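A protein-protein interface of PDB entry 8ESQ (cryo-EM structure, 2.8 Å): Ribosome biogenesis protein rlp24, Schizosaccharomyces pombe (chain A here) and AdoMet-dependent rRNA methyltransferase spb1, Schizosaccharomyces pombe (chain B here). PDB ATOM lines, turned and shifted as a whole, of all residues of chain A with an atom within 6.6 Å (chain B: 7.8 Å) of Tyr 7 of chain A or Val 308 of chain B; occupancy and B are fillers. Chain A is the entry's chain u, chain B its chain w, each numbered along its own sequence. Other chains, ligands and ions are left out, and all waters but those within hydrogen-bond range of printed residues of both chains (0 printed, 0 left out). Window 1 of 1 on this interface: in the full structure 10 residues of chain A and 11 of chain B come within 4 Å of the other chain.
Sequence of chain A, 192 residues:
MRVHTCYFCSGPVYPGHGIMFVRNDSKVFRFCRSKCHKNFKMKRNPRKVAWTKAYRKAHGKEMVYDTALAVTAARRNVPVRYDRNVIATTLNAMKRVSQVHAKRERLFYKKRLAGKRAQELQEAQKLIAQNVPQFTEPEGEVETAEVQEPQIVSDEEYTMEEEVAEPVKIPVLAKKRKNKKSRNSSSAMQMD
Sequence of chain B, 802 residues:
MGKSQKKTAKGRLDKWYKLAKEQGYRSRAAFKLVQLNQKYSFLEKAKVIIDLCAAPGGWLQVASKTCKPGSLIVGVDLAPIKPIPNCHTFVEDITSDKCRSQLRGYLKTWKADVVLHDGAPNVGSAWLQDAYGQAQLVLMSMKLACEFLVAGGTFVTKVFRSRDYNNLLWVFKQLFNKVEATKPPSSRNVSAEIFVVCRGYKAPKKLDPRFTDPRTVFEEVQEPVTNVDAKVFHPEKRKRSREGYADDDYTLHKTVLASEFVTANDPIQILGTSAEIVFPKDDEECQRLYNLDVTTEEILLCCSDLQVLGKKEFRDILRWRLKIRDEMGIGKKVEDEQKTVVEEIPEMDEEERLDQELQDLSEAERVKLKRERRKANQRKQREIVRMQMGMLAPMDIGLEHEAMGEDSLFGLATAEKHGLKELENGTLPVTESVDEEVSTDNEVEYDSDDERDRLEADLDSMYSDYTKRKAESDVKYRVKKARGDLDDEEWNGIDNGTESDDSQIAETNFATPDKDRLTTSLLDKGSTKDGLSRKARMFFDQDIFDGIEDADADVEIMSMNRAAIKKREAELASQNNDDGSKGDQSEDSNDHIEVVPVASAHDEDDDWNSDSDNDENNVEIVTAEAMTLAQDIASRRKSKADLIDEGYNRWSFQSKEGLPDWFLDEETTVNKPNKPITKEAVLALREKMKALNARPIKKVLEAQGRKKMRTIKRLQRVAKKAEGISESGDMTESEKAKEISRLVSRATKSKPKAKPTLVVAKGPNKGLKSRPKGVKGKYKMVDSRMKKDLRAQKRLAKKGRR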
ATOM      1  N   THR A   5      17.529 -14.059  20.953  1.00  0.00           N
ATOM      2  CA  THR A   5      17.833 -13.872  19.542  1.00  0.00           C
ATOM      3  C   THR A   5      18.104 -12.394  19.302  1.00  0.00           C
ATOM      4  O   THR A   5      17.310 -11.542  19.711  1.00  0.00           O
ATOM      5  CB  THR A   5      16.683 -14.355  18.658  1.00  0.00           C
ATOM      6  OG1 THR A   5      15.523 -13.549  18.898  1.00  0.00           O
ATOM      7  CG2 THR A   5      16.355 -15.808  18.962  1.00  0.00           C
ATOM      8  N   CYS A   6      19.228 -12.098  18.655  1.00  0.00           N
ATOM      9  CA  CYS A   6      19.559 -10.717  18.333  1.00  0.00           C
ATOM     10  C   CYS A   6      18.481 -10.119  17.441  1.00  0.00           C
ATOM     11  O   CYS A   6      17.882 -10.811  16.616  1.00  0.00           O
ATOM     12  CB  CYS A   6      20.921 -10.647  17.642  1.00  0.00           C
ATOM     13  SG  CYS A   6      21.265  -9.084  16.805  1.00  0.00           S
ATOM     14  N   TYR A   7      18.198  -8.829  17.637  1.00  0.00           N
ATOM     15  CA  TYR A   7      17.194  -8.186  16.797  1.00  0.00           C
ATOM     16  C   TYR A   7      17.659  -8.122  15.349  1.00  0.00           C
ATOM     17  O   TYR A   7      16.874  -8.356  14.424  1.00  0.00           O
ATOM     18  CB  TYR A   7      16.875  -6.781  17.311  1.00  0.00           C
ATOM     19  CG  TYR A   7      16.582  -5.793  16.200  1.00  0.00           C
ATOM     20  CD1 TYR A   7      15.295  -5.658  15.696  1.00  0.00           C
ATOM     21  CD2 TYR A   7      17.587  -5.010  15.641  1.00  0.00           C
ATOM     22  CE1 TYR A   7      15.014  -4.771  14.678  1.00  0.00           C
ATOM     23  CE2 TYR A   7      17.316  -4.128  14.617  1.00  0.00           C
ATOM     24  CZ  TYR A   7      16.028  -4.005  14.144  1.00  0.00           C
ATOM     25  OH  TYR A   7      15.749  -3.122  13.127  1.00  0.00           O
ATOM     26  N   PHE A   8      18.935  -7.805  15.136  1.00  0.00           N
ATOM     27  CA  PHE A   8      19.448  -7.505  13.803  1.00  0.00           C
ATOM     28  C   PHE A   8      19.904  -8.765  13.074  1.00  0.00           C
ATOM     29  O   PHE A   8      19.371  -9.105  12.014  1.00  0.00           O
ATOM     30  CB  PHE A   8      20.599  -6.500  13.909  1.00  0.00           C
ATOM     31  CG  PHE A   8      20.777  -5.657  12.688  1.00  0.00           C
ATOM     32  CD1 PHE A   8      21.595  -6.073  11.652  1.00  0.00           C
ATOM     33  CD2 PHE A   8      20.120  -4.447  12.572  1.00  0.00           C
ATOM     34  CE1 PHE A   8      21.756  -5.294  10.525  1.00  0.00           C
ATOM     35  CE2 PHE A   8      20.277  -3.663  11.451  1.00  0.00           C
ATOM     36  CZ  PHE A   8      21.092  -4.088  10.423  1.00  0.00           C
ATOM     37  N   CYS A   9      20.891  -9.464  13.631  1.00  0.00           N
ATOM     38  CA  CYS A   9      21.405 -10.681  13.019  1.00  0.00           C
ATOM     39  C   CYS A   9      20.480 -11.873  13.204  1.00  0.00           C
ATOM     40  O   CYS A   9      20.658 -12.883  12.517  1.00  0.00           O
ATOM     41  CB  CYS A   9      22.782 -11.016  13.597  1.00  0.00           C
ATOM     42  SG  CYS A   9      23.773 -12.147  12.595  1.00  0.00           S
ATOM     43  N   SER A  10      19.510 -11.781  14.114  1.00  0.00           N
ATOM     44  CA  SER A  10      18.654 -12.900  14.500  1.00  0.00           C
ATOM     45  C   SER A  10      19.466 -14.094  14.984  1.00  0.00           C
ATOM     46  O   SER A  10      18.995 -15.233  14.928  1.00  0.00           O
ATOM     47  CB  SER A  10      17.722 -13.313  13.357  1.00  0.00           C
ATOM     48  OG  SER A  10      16.674 -12.374  13.194  1.00  0.00           O
ATOM     49  N   GLY A  11      20.680 -13.830  15.458  1.00  0.00           N
ATOM     50  CA  GLY A  11      21.538 -14.899  15.935  1.00  0.00           C
ATOM     51  C   GLY A  11      21.422 -15.147  17.423  1.00  0.00           C
ATOM     52  O   GLY A  11      20.748 -14.398  18.130  1.00  0.00           O
ATOM     53  N   VAL A  13      22.062 -15.002  21.212  1.00  0.00           N
ATOM     54  CA  VAL A  13      22.705 -14.094  22.154  1.00  0.00           C
ATOM     55  C   VAL A  13      22.748 -14.787  23.507  1.00  0.00           C
ATOM     56  O   VAL A  13      21.704 -15.159  24.057  1.00  0.00           O
ATOM     57  CB  VAL A  13      21.968 -12.750  22.244  1.00  0.00           C
ATOM     58  CG1 VAL A  13      22.620 -11.858  23.287  1.00  0.00           C
ATOM     59  CG2 VAL A  13      21.948 -12.068  20.891  1.00  0.00           C
ATOM     60  N   ARG A  23      13.924   0.780  24.422  1.00  0.00           N
ATOM     61  CA  ARG A  23      13.335   1.936  23.765  1.00  0.00           C
ATOM     62  C   ARG A  23      12.221   2.536  24.621  1.00  0.00           C
ATOM     63  O   ARG A  23      11.695   1.894  25.532  1.00  0.00           O
ATOM     64  CB  ARG A  23      12.805   1.548  22.384  1.00  0.00           C
ATOM     65  CG  ARG A  23      12.799   2.675  21.370  1.00  0.00           C
ATOM     66  CD  ARG A  23      12.750   2.122  19.958  1.00  0.00           C
ATOM     67  NE  ARG A  23      11.679   1.147  19.785  1.00  0.00           N
ATOM     68  CZ  ARG A  23      11.097   0.876  18.625  1.00  0.00           C
ATOM     69  NH1 ARG A  23      11.463   1.484  17.509  1.00  0.00           N
ATOM     70  NH2 ARG A  23      10.128  -0.035  18.583  1.00  0.00           N
ATOM     71  N   VAL A  28      12.486  -3.952  23.729  1.00  0.00           N
ATOM     72  CA  VAL A  28      13.859  -4.309  24.056  1.00  0.00           C
ATOM     73  C   VAL A  28      14.537  -4.837  22.802  1.00  0.00           C
ATOM     74  O   VAL A  28      14.038  -5.770  22.159  1.00  0.00           O
ATOM     75  CB  VAL A  28      13.914  -5.346  25.185  1.00  0.00           C
ATOM     76  CG1 VAL A  28      15.323  -5.465  25.707  1.00  0.00           C
ATOM     77  CG2 VAL A  28      12.956  -4.962  26.301  1.00  0.00           C
ATOM     78  N   PHE A  29      15.670  -4.236  22.450  1.00  0.00           N
ATOM     79  CA  PHE A  29      16.516  -4.705  21.361  1.00  0.00           C
ATOM     80  C   PHE A  29      17.781  -5.307  21.957  1.00  0.00           C
ATOM     81  O   PHE A  29      18.506  -4.631  22.695  1.00  0.00           O
ATOM     82  CB  PHE A  29      16.865  -3.567  20.403  1.00  0.00           C
ATOM     83  CG  PHE A  29      15.669  -2.892  19.803  1.00  0.00           C
ATOM     84  CD1 PHE A  29      14.974  -3.483  18.763  1.00  0.00           C
ATOM     85  CD2 PHE A  29      15.238  -1.666  20.280  1.00  0.00           C
ATOM     86  CE1 PHE A  29      13.874  -2.863  18.206  1.00  0.00           C
ATOM     87  CE2 PHE A  29      14.138  -1.044  19.730  1.00  0.00           C
ATOM     88  CZ  PHE A  29      13.455  -1.642  18.691  1.00  0.00           C
ATOM     89  N   ARG A  30      18.040  -6.569  21.637  1.00  0.00           N
ATOM     90  CA  ARG A  30      19.242  -7.268  22.072  1.00  0.00           C
ATOM     91  C   ARG A  30      20.133  -7.481  20.858  1.00  0.00           C
ATOM     92  O   ARG A  30      19.663  -7.949  19.817  1.00  0.00           O
ATOM     93  CB  ARG A  30      18.891  -8.599  22.734  1.00  0.00           C
ATOM     94  CG  ARG A  30      17.927  -8.461  23.894  1.00  0.00           C
ATOM     95  CD  ARG A  30      17.298  -9.791  24.247  1.00  0.00           C
ATOM     96  NE  ARG A  30      16.253  -9.645  25.252  1.00  0.00           N
ATOM     97  CZ  ARG A  30      16.413  -9.913  26.539  1.00  0.00           C
ATOM     98  NH1 ARG A  30      17.570 -10.342  27.017  1.00  0.00           N
ATOM     99  NH2 ARG A  30      15.388  -9.747  27.369  1.00  0.00           N
ATOM    100  N   PHE A  31      21.406  -7.124  20.988  1.00  0.00           N
ATOM    101  CA  PHE A  31      22.363  -7.213  19.896  1.00  0.00           C
ATOM    102  C   PHE A  31      23.438  -8.230  20.245  1.00  0.00           C
ATOM    103  O   PHE A  31      23.959  -8.229  21.364  1.00  0.00           O
ATOM    104  CB  PHE A  31      22.986  -5.847  19.613  1.00  0.00           C
ATOM    105  CG  PHE A  31      21.976  -4.760  19.419  1.00  0.00           C
ATOM    106  CD1 PHE A  31      21.005  -4.868  18.440  1.00  0.00           C
ATOM    107  CD2 PHE A  31      21.987  -3.635  20.225  1.00  0.00           C
ATOM    108  CE1 PHE A  31      20.070  -3.871  18.263  1.00  0.00           C
ATOM    109  CE2 PHE A  31      21.054  -2.635  20.052  1.00  0.00           C
ATOM    110  CZ  PHE A  31      20.095  -2.754  19.071  1.00  0.00           C
ATOM    111  N   CYS A  32      23.760  -9.101  19.289  1.00  0.00           N
ATOM    112  CA  CYS A  32      24.751 -10.142  19.527  1.00  0.00           C
ATOM    113  C   CYS A  32      26.179  -9.614  19.512  1.00  0.00           C
ATOM    114  O   CYS A  32      27.068 -10.264  20.070  1.00  0.00           O
ATOM    115  CB  CYS A  32      24.596 -11.254  18.490  1.00  0.00           C
ATOM    116  SG  CYS A  32      24.713 -10.686  16.784  1.00  0.00           S
ATOM    117  N   CYS A  36      26.319  -5.521  14.842  1.00  0.00           N
ATOM    118  CA  CYS A  36      24.864  -5.471  14.755  1.00  0.00           C
ATOM    119  C   CYS A  36      24.303  -4.282  15.524  1.00  0.00           C
ATOM    120  O   CYS A  36      23.329  -3.659  15.088  1.00  0.00           O
ATOM    121  CB  CYS A  36      24.266  -6.779  15.266  1.00  0.00           C
ATOM    122  SG  CYS A  36      24.834  -8.231  14.361  1.00  0.00           S
ATOM    123  N   ASN A  39      24.779  -1.218  13.469  1.00  0.00           N
ATOM    124  CA  ASN A  39      23.875  -1.267  12.325  1.00  0.00           C
ATOM    125  C   ASN A  39      22.463  -0.860  12.724  1.00  0.00           C
ATOM    126  O   ASN A  39      21.761  -0.193  11.955  1.00  0.00           O
ATOM    127  CB  ASN A  39      23.897  -2.663  11.710  1.00  0.00           C
ATOM    128  CG  ASN A  39      25.154  -2.917  10.908  1.00  0.00           C
ATOM    129  OD1 ASN A  39      25.946  -2.004  10.674  1.00  0.00           O
ATOM    130  ND2 ASN A  39      25.352  -4.158  10.491  1.00  0.00           N
ATOM    131  N   PHE A  40      22.025  -1.259  13.919  1.00  0.00           N
ATOM    132  CA  PHE A  40      20.784  -0.721  14.465  1.00  0.00           C
ATOM    133  C   PHE A  40      20.886   0.784  14.673  1.00  0.00           C
ATOM    134  O   PHE A  40      19.904   1.511  14.489  1.00  0.00           O
ATOM    135  CB  PHE A  40      20.440  -1.420  15.781  1.00  0.00           C
ATOM    136  CG  PHE A  40      19.215  -0.870  16.465  1.00  0.00           C
ATOM    137  CD1 PHE A  40      19.317   0.181  17.361  1.00  0.00           C
ATOM    138  CD2 PHE A  40      17.966  -1.404  16.215  1.00  0.00           C
ATOM    139  CE1 PHE A  40      18.194   0.686  17.988  1.00  0.00           C
ATOM    140  CE2 PHE A  40      16.843  -0.906  16.841  1.00  0.00           C
ATOM    141  CZ  PHE A  40      16.956   0.141  17.727  1.00  0.00           C
ATOM    142  N   LYS A  43      20.352   2.395  11.777  1.00  0.00           N
ATOM    143  CA  LYS A  43      18.980   2.042  11.429  1.00  0.00           C
ATOM    144  C   LYS A  43      18.886   1.361  10.068  1.00  0.00           C
ATOM    145  O   LYS A  43      17.908   1.544   9.340  1.00  0.00           O
ATOM    146  CB  LYS A  43      18.062   3.266  11.483  1.00  0.00           C
ATOM    147  CG  LYS A  43      18.115   4.005  12.812  1.00  0.00           C
ATOM    148  CD  LYS A  43      17.138   5.163  12.838  1.00  0.00           C
ATOM    149  CE  LYS A  43      17.217   5.932  14.145  1.00  0.00           C
ATOM    150  NZ  LYS A  43      16.307   7.113  14.138  1.00  0.00           N
ATOM    151  N   ARG A  44      19.901   0.579   9.711  1.00  0.00           N
ATOM    152  CA  ARG A  44      19.844  -0.206   8.489  1.00  0.00           C
ATOM    153  C   ARG A  44      18.792  -1.302   8.617  1.00  0.00           C
ATOM    154  O   ARG A  44      18.575  -1.864   9.693  1.00  0.00           O
ATOM    155  CB  ARG A  44      21.213  -0.811   8.187  1.00  0.00           C
ATOM    156  CG  ARG A  44      22.317   0.225   8.055  1.00  0.00           C
ATOM    157  CD  ARG A  44      23.650  -0.413   7.708  1.00  0.00           C
ATOM    158  NE  ARG A  44      24.699   0.586   7.550  1.00  0.00           N
ATOM    159  CZ  ARG A  44      25.146   1.025   6.381  1.00  0.00           C
ATOM    160  NH1 ARG A  44      24.659   0.567   5.239  1.00  0.00           N
ATOM    161  NH2 ARG A  44      26.102   1.949   6.357  1.00  0.00           N
ATOM    162  N   ASN A  45      18.125  -1.593   7.511  1.00  0.00           N
ATOM    163  CA  ASN A  45      17.064  -2.594   7.534  1.00  0.00           C
ATOM    164  C   ASN A  45      17.670  -3.993   7.500  1.00  0.00           C
ATOM    165  O   ASN A  45      18.458  -4.297   6.598  1.00  0.00           O
ATOM    166  CB  ASN A  45      16.115  -2.394   6.358  1.00  0.00           C
ATOM    167  CG  ASN A  45      15.131  -3.533   6.200  1.00  0.00           C
ATOM    168  OD1 ASN A  45      15.434  -4.545   5.573  1.00  0.00           O
ATOM    169  ND2 ASN A  45      13.944  -3.375   6.775  1.00  0.00           N
ATOM    170  N   PRO A  46      17.340  -4.859   8.463  1.00  0.00           N
ATOM    171  CA  PRO A  46      17.944  -6.207   8.469  1.00  0.00           C
ATOM    172  C   PRO A  46      17.688  -6.997   7.196  1.00  0.00           C
ATOM    173  O   PRO A  46      18.597  -7.676   6.701  1.00  0.00           O
ATOM    174  CB  PRO A  46      17.303  -6.870   9.699  1.00  0.00           C
ATOM    175  CG  PRO A  46      16.112  -6.025  10.037  1.00  0.00           C
ATOM    176  CD  PRO A  46      16.463  -4.637   9.622  1.00  0.00           C
ATOM    177  N   ALA A  54      17.188 -12.232   8.527  1.00  0.00           N
ATOM    178  CA  ALA A  54      15.960 -11.706   7.940  1.00  0.00           C
ATOM    179  C   ALA A  54      16.082 -11.579   6.427  1.00  0.00           C
ATOM    180  O   ALA A  54      15.132 -11.871   5.693  1.00  0.00           O
ATOM    181  CB  ALA A  54      15.614 -10.356   8.567  1.00  0.00           C
ATOM    182  N   PRO B 235      18.566  10.164  10.576  1.00  0.00           N
ATOM    183  CA  PRO B 235      18.540   9.214  11.699  1.00  0.00           C
ATOM    184  C   PRO B 235      19.742   9.347  12.616  1.00  0.00           C
ATOM    185  O   PRO B 235      19.665   8.954  13.786  1.00  0.00           O
ATOM    186  CB  PRO B 235      18.511   7.847  11.003  1.00  0.00           C
ATOM    187  CG  PRO B 235      19.060   8.098   9.638  1.00  0.00           C
ATOM    188  CD  PRO B 235      18.631   9.485   9.272  1.00  0.00           C
ATOM    189  N   ALA B 275       5.828   8.014  16.967  1.00  0.00           N
ATOM    190  CA  ALA B 275       6.717   6.861  17.049  1.00  0.00           C
ATOM    191  C   ALA B 275       6.436   5.858  15.939  1.00  0.00           C
ATOM    192  O   ALA B 275       7.357   5.182  15.467  1.00  0.00           O
ATOM    193  CB  ALA B 275       6.587   6.192  18.416  1.00  0.00           C
ATOM    194  N   GLU B 298       7.430  -4.395   3.052  1.00  0.00           N
ATOM    195  CA  GLU B 298       8.463  -3.517   3.589  1.00  0.00           C
ATOM    196  C   GLU B 298       7.858  -2.224   4.120  1.00  0.00           C
ATOM    197  O   GLU B 298       8.233  -1.748   5.197  1.00  0.00           O
ATOM    198  CB  GLU B 298       9.511  -3.221   2.515  1.00  0.00           C
ATOM    199  CG  GLU B 298      10.617  -2.276   2.962  1.00  0.00           C
ATOM    200  CD  GLU B 298      11.504  -2.877   4.035  1.00  0.00           C
ATOM    201  OE1 GLU B 298      11.648  -4.118   4.065  1.00  0.00           O
ATOM    202  OE2 GLU B 298      12.058  -2.109   4.849  1.00  0.00           O
ATOM    203  N   LEU B 301       6.187  -2.994   7.332  1.00  0.00           N
ATOM    204  CA  LEU B 301       7.206  -3.105   8.371  1.00  0.00           C
ATOM    205  C   LEU B 301       7.776  -1.738   8.731  1.00  0.00           C
ATOM    206  O   LEU B 301       8.047  -1.460   9.906  1.00  0.00           O
ATOM    207  CB  LEU B 301       8.319  -4.050   7.916  1.00  0.00           C
ATOM    208  CG  LEU B 301       9.435  -4.305   8.930  1.00  0.00           C
ATOM    209  CD1 LEU B 301       8.877  -4.947  10.190  1.00  0.00           C
ATOM    210  CD2 LEU B 301      10.526  -5.170   8.321  1.00  0.00           C
ATOM    211  N   CYS B 302       7.974  -0.875   7.731  1.00  0.00           N
ATOM    212  CA  CYS B 302       8.473   0.469   8.001  1.00  0.00           C
ATOM    213  C   CYS B 302       7.494   1.259   8.861  1.00  0.00           C
ATOM    214  O   CYS B 302       7.903   1.962   9.793  1.00  0.00           O
ATOM    215  CB  CYS B 302       8.743   1.202   6.687  1.00  0.00           C
ATOM    216  SG  CYS B 302      10.172   0.599   5.755  1.00  0.00           S
ATOM    217  N   SER B 304       5.273  -0.038  10.881  1.00  0.00           N
ATOM    218  CA  SER B 304       5.196  -0.676  12.191  1.00  0.00           C
ATOM    219  C   SER B 304       6.292  -0.166  13.119  1.00  0.00           C
ATOM    220  O   SER B 304       6.058   0.035  14.316  1.00  0.00           O
ATOM    221  CB  SER B 304       5.280  -2.195  12.043  1.00  0.00           C
ATOM    222  OG  SER B 304       6.571  -2.597  11.621  1.00  0.00           O
ATOM    223  N   ASP B 305       7.499   0.044  12.588  1.00  0.00           N
ATOM    224  CA  ASP B 305       8.623   0.586  13.356  1.00  0.00           C
ATOM    225  C   ASP B 305       9.197   1.767  12.576  1.00  0.00           C
ATOM    226  O   ASP B 305      10.141   1.616  11.797  1.00  0.00           O
ATOM    227  CB  ASP B 305       9.677  -0.488  13.625  1.00  0.00           C
ATOM    228  CG  ASP B 305      10.588  -0.133  14.785  1.00  0.00           C
ATOM    229  OD1 ASP B 305      10.906   1.063  14.951  1.00  0.00           O
ATOM    230  OD2 ASP B 305      10.987  -1.051  15.532  1.00  0.00           O
ATOM    231  N   LEU B 306       8.616   2.950  12.790  1.00  0.00           N
ATOM    232  CA  LEU B 306       9.133   4.152  12.145  1.00  0.00           C
ATOM    233  C   LEU B 306      10.499   4.535  12.697  1.00  0.00           C
ATOM    234  O   LEU B 306      11.374   4.981  11.946  1.00  0.00           O
ATOM    235  CB  LEU B 306       8.157   5.313  12.323  1.00  0.00           C
ATOM    236  CG  LEU B 306       6.920   5.379  11.434  1.00  0.00           C
ATOM    237  CD1 LEU B 306       6.211   6.699  11.672  1.00  0.00           C
ATOM    238  CD2 LEU B 306       7.294   5.223   9.971  1.00  0.00           C
ATOM    239  N   GLN B 307      10.696   4.377  14.007  1.00  0.00           N
ATOM    240  CA  GLN B 307      11.907   4.886  14.641  1.00  0.00           C
ATOM    241  C   GLN B 307      13.155   4.194  14.108  1.00  0.00           C
ATOM    242  O   GLN B 307      14.185   4.841  13.894  1.00  0.00           O
ATOM    243  CB  GLN B 307      11.804   4.738  16.158  1.00  0.00           C
ATOM    244  CG  GLN B 307      10.809   5.702  16.786  1.00  0.00           C
ATOM    245  CD  GLN B 307      10.744   5.584  18.292  1.00  0.00           C
ATOM    246  OE1 GLN B 307      11.382   4.718  18.887  1.00  0.00           O
ATOM    247  NE2 GLN B 307       9.969   6.460  18.920  1.00  0.00           N
ATOM    248  N   VAL B 308      13.088   2.885  13.886  1.00  0.00           N
ATOM    249  CA  VAL B 308      14.231   2.146  13.322  1.00  0.00           C
ATOM    250  C   VAL B 308      14.060   2.192  11.809  1.00  0.00           C
ATOM    251  O   VAL B 308      13.604   1.246  11.163  1.00  0.00           O
ATOM    252  CB  VAL B 308      14.320   0.717  13.865  1.00  0.00           C
ATOM    253  CG1 VAL B 308      15.663   0.100  13.509  1.00  0.00           C
ATOM    254  CG2 VAL B 308      14.101   0.709  15.367  1.00  0.00           C
ATOM    255  N   LEU B 309      14.478   3.313  11.221  1.00  0.00           N
ATOM    256  CA  LEU B 309      14.381   3.532   9.785  1.00  0.00           C
ATOM    257  C   LEU B 309      15.379   4.608   9.387  1.00  0.00           C
ATOM    258  O   LEU B 309      15.526   5.613  10.089  1.00  0.00           O
ATOM    259  CB  LEU B 309      12.968   3.955   9.359  1.00  0.00           C
ATOM    260  CG  LEU B 309      11.866   2.901   9.225  1.00  0.00           C
ATOM    261  CD1 LEU B 309      10.581   3.530   8.716  1.00  0.00           C
ATOM    262  CD2 LEU B 309      12.311   1.766   8.318  1.00  0.00           C
ATOM    263  N   GLY B 310      16.053   4.397   8.256  1.00  0.00           N
ATOM    264  CA  GLY B 310      17.011   5.356   7.751  1.00  0.00           C
ATOM    265  C   GLY B 310      16.365   6.433   6.898  1.00  0.00           C
ATOM    266  O   GLY B 310      15.146   6.508   6.747  1.00  0.00           O
ATOM    267  N   GLU B 313      14.588   4.886   3.769  1.00  0.00           N
ATOM    268  CA  GLU B 313      13.314   4.257   4.102  1.00  0.00           C
ATOM    269  C   GLU B 313      12.231   5.296   4.364  1.00  0.00           C
ATOM    270  O   GLU B 313      11.080   5.119   3.947  1.00  0.00           O
ATOM    271  CB  GLU B 313      13.486   3.333   5.307  1.00  0.00           C
ATOM    272  CG  GLU B 313      14.302   2.079   5.022  1.00  0.00           C
ATOM    273  CD  GLU B 313      15.799   2.324   5.056  1.00  0.00           C
ATOM    274  OE1 GLU B 313      16.211   3.465   5.348  1.00  0.00           O
ATOM    275  OE2 GLU B 313      16.564   1.374   4.792  1.00  0.00           O
ATOM    276  N   PHE B 314      12.576   6.385   5.056  1.00  0.00           N
ATOM    277  CA  PHE B 314      11.612   7.463   5.257  1.00  0.00           C
ATOM    278  C   PHE B 314      11.194   8.087   3.932  1.00  0.00           C
ATOM    279  O   PHE B 314      10.012   8.385   3.726  1.00  0.00           O
ATOM    280  CB  PHE B 314      12.187   8.524   6.193  1.00  0.00           C
ATOM    281  CG  PHE B 314      12.047   8.190   7.651  1.00  0.00           C
ATOM    282  CD1 PHE B 314      11.156   7.219   8.070  1.00  0.00           C
ATOM    283  CD2 PHE B 314      12.802   8.853   8.601  1.00  0.00           C
ATOM    284  CE1 PHE B 314      11.022   6.918   9.411  1.00  0.00           C
ATOM    285  CE2 PHE B 314      12.675   8.554   9.942  1.00  0.00           C
ATOM    286  CZ  PHE B 314      11.784   7.585  10.347  1.00  0.00           C
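Of the 22 printed residues of chain A, 5 touch a printed residue of chain B. Among the printed residues, Asp or Glu carboxylates within 4 Å of a Lys or Arg side-chain nitrogen of the other chain: Arg 23 of chain A with Asp 305 of chain B (2.7 Å).
Tyr 7 of chain A touches just one residue of chain B: Val 308 (3.2 Å). Of the printed residues of chain A, Val 308 of chain B touches Tyr 7 (3.2 Å), Arg 23 (3.5 Å) and Phe 40 (3.5 Å). No residue of chain B comes within 4 Å of Cys 6 of chain A. Of the printed residues of chain A, Glu 298 of chain B touches Asn 45 (3.0 Å). Printed residues of chain B within 4 Å of Lys 43 of chain A: Pro 235, Gln 307, Leu 309 and Gly 310. Of the printed residues of chain A, Pro 235 of chain B touches Lys 43. Phe 31 of chain A touches none of the printed residues of chain B. The nearest residue of chain B that does not touch Tyr 7 of chain A is Asp 305 of chain B (5.5 Å). The nearest residue of chain A that does not touch Val 308 of chain B is Phe 29 of chain A (4.1 Å).
The backbone NH (N) of Tyr 7 of chain A lies within hydrogen-bond range of the backbone carbonyl oxygen (O) of Arg 30 of chain A (2.8 Å). SG of Cys 302 of chain B lies within hydrogen-bond range of O of Glu 298 of chain B (3.1 Å). The backbone NH (N) of Gln 307 of chain B sits close to the side-chain carboxylate (OD1) of Asp 305 of chain B, 3.5 Å away. OD1 of Asp 305 of chain B is in hydrogen-bond range of N of Val 308 of chain B (3.0 Å). N of Gly 310 of chain B lies within hydrogen-bond range of OE1 of Glu 313 of chain B, at 3.1 Å.
The guanidinium group (NH1) of Arg 23 of chain A is in salt-bridge range of the side-chain carboxylate (OD1) of Asp 305 of chain B, 2.7 Å away. The backbone carbonyl oxygen (O) of Gln 307 of chain B lies within hydrogen-bond range of the side-chain amino group (NZ) of Lys 43 of chain A, at 3.1 Å. The side-chain amide nitrogen of Asn 45 of chain A lies within hydrogen-bond range of the side-chain carboxylate of Glu 298 of chain B.
CG1 of Val 308 of chain B touches OH of Tyr 7 of chain A (3.2 Å). OE1 of Gln 307 of chain B touches CD of Arg 23 of chain A (3.1 Å). Arg 23 of chain A touches Val 308 of chain B. CE2 of Phe 40 of chain A touches CG2 of Val 308 of chain B, at 3.5 Å. CD of Lys 43 of chain A touches CB of Pro 235 of chain B (3.5 Å). CD of Lys 43 of chain A touches O of Leu 309 of chain B, 3.2 Å away. Gly 310 of chain B touches Lys 43 of chain A.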
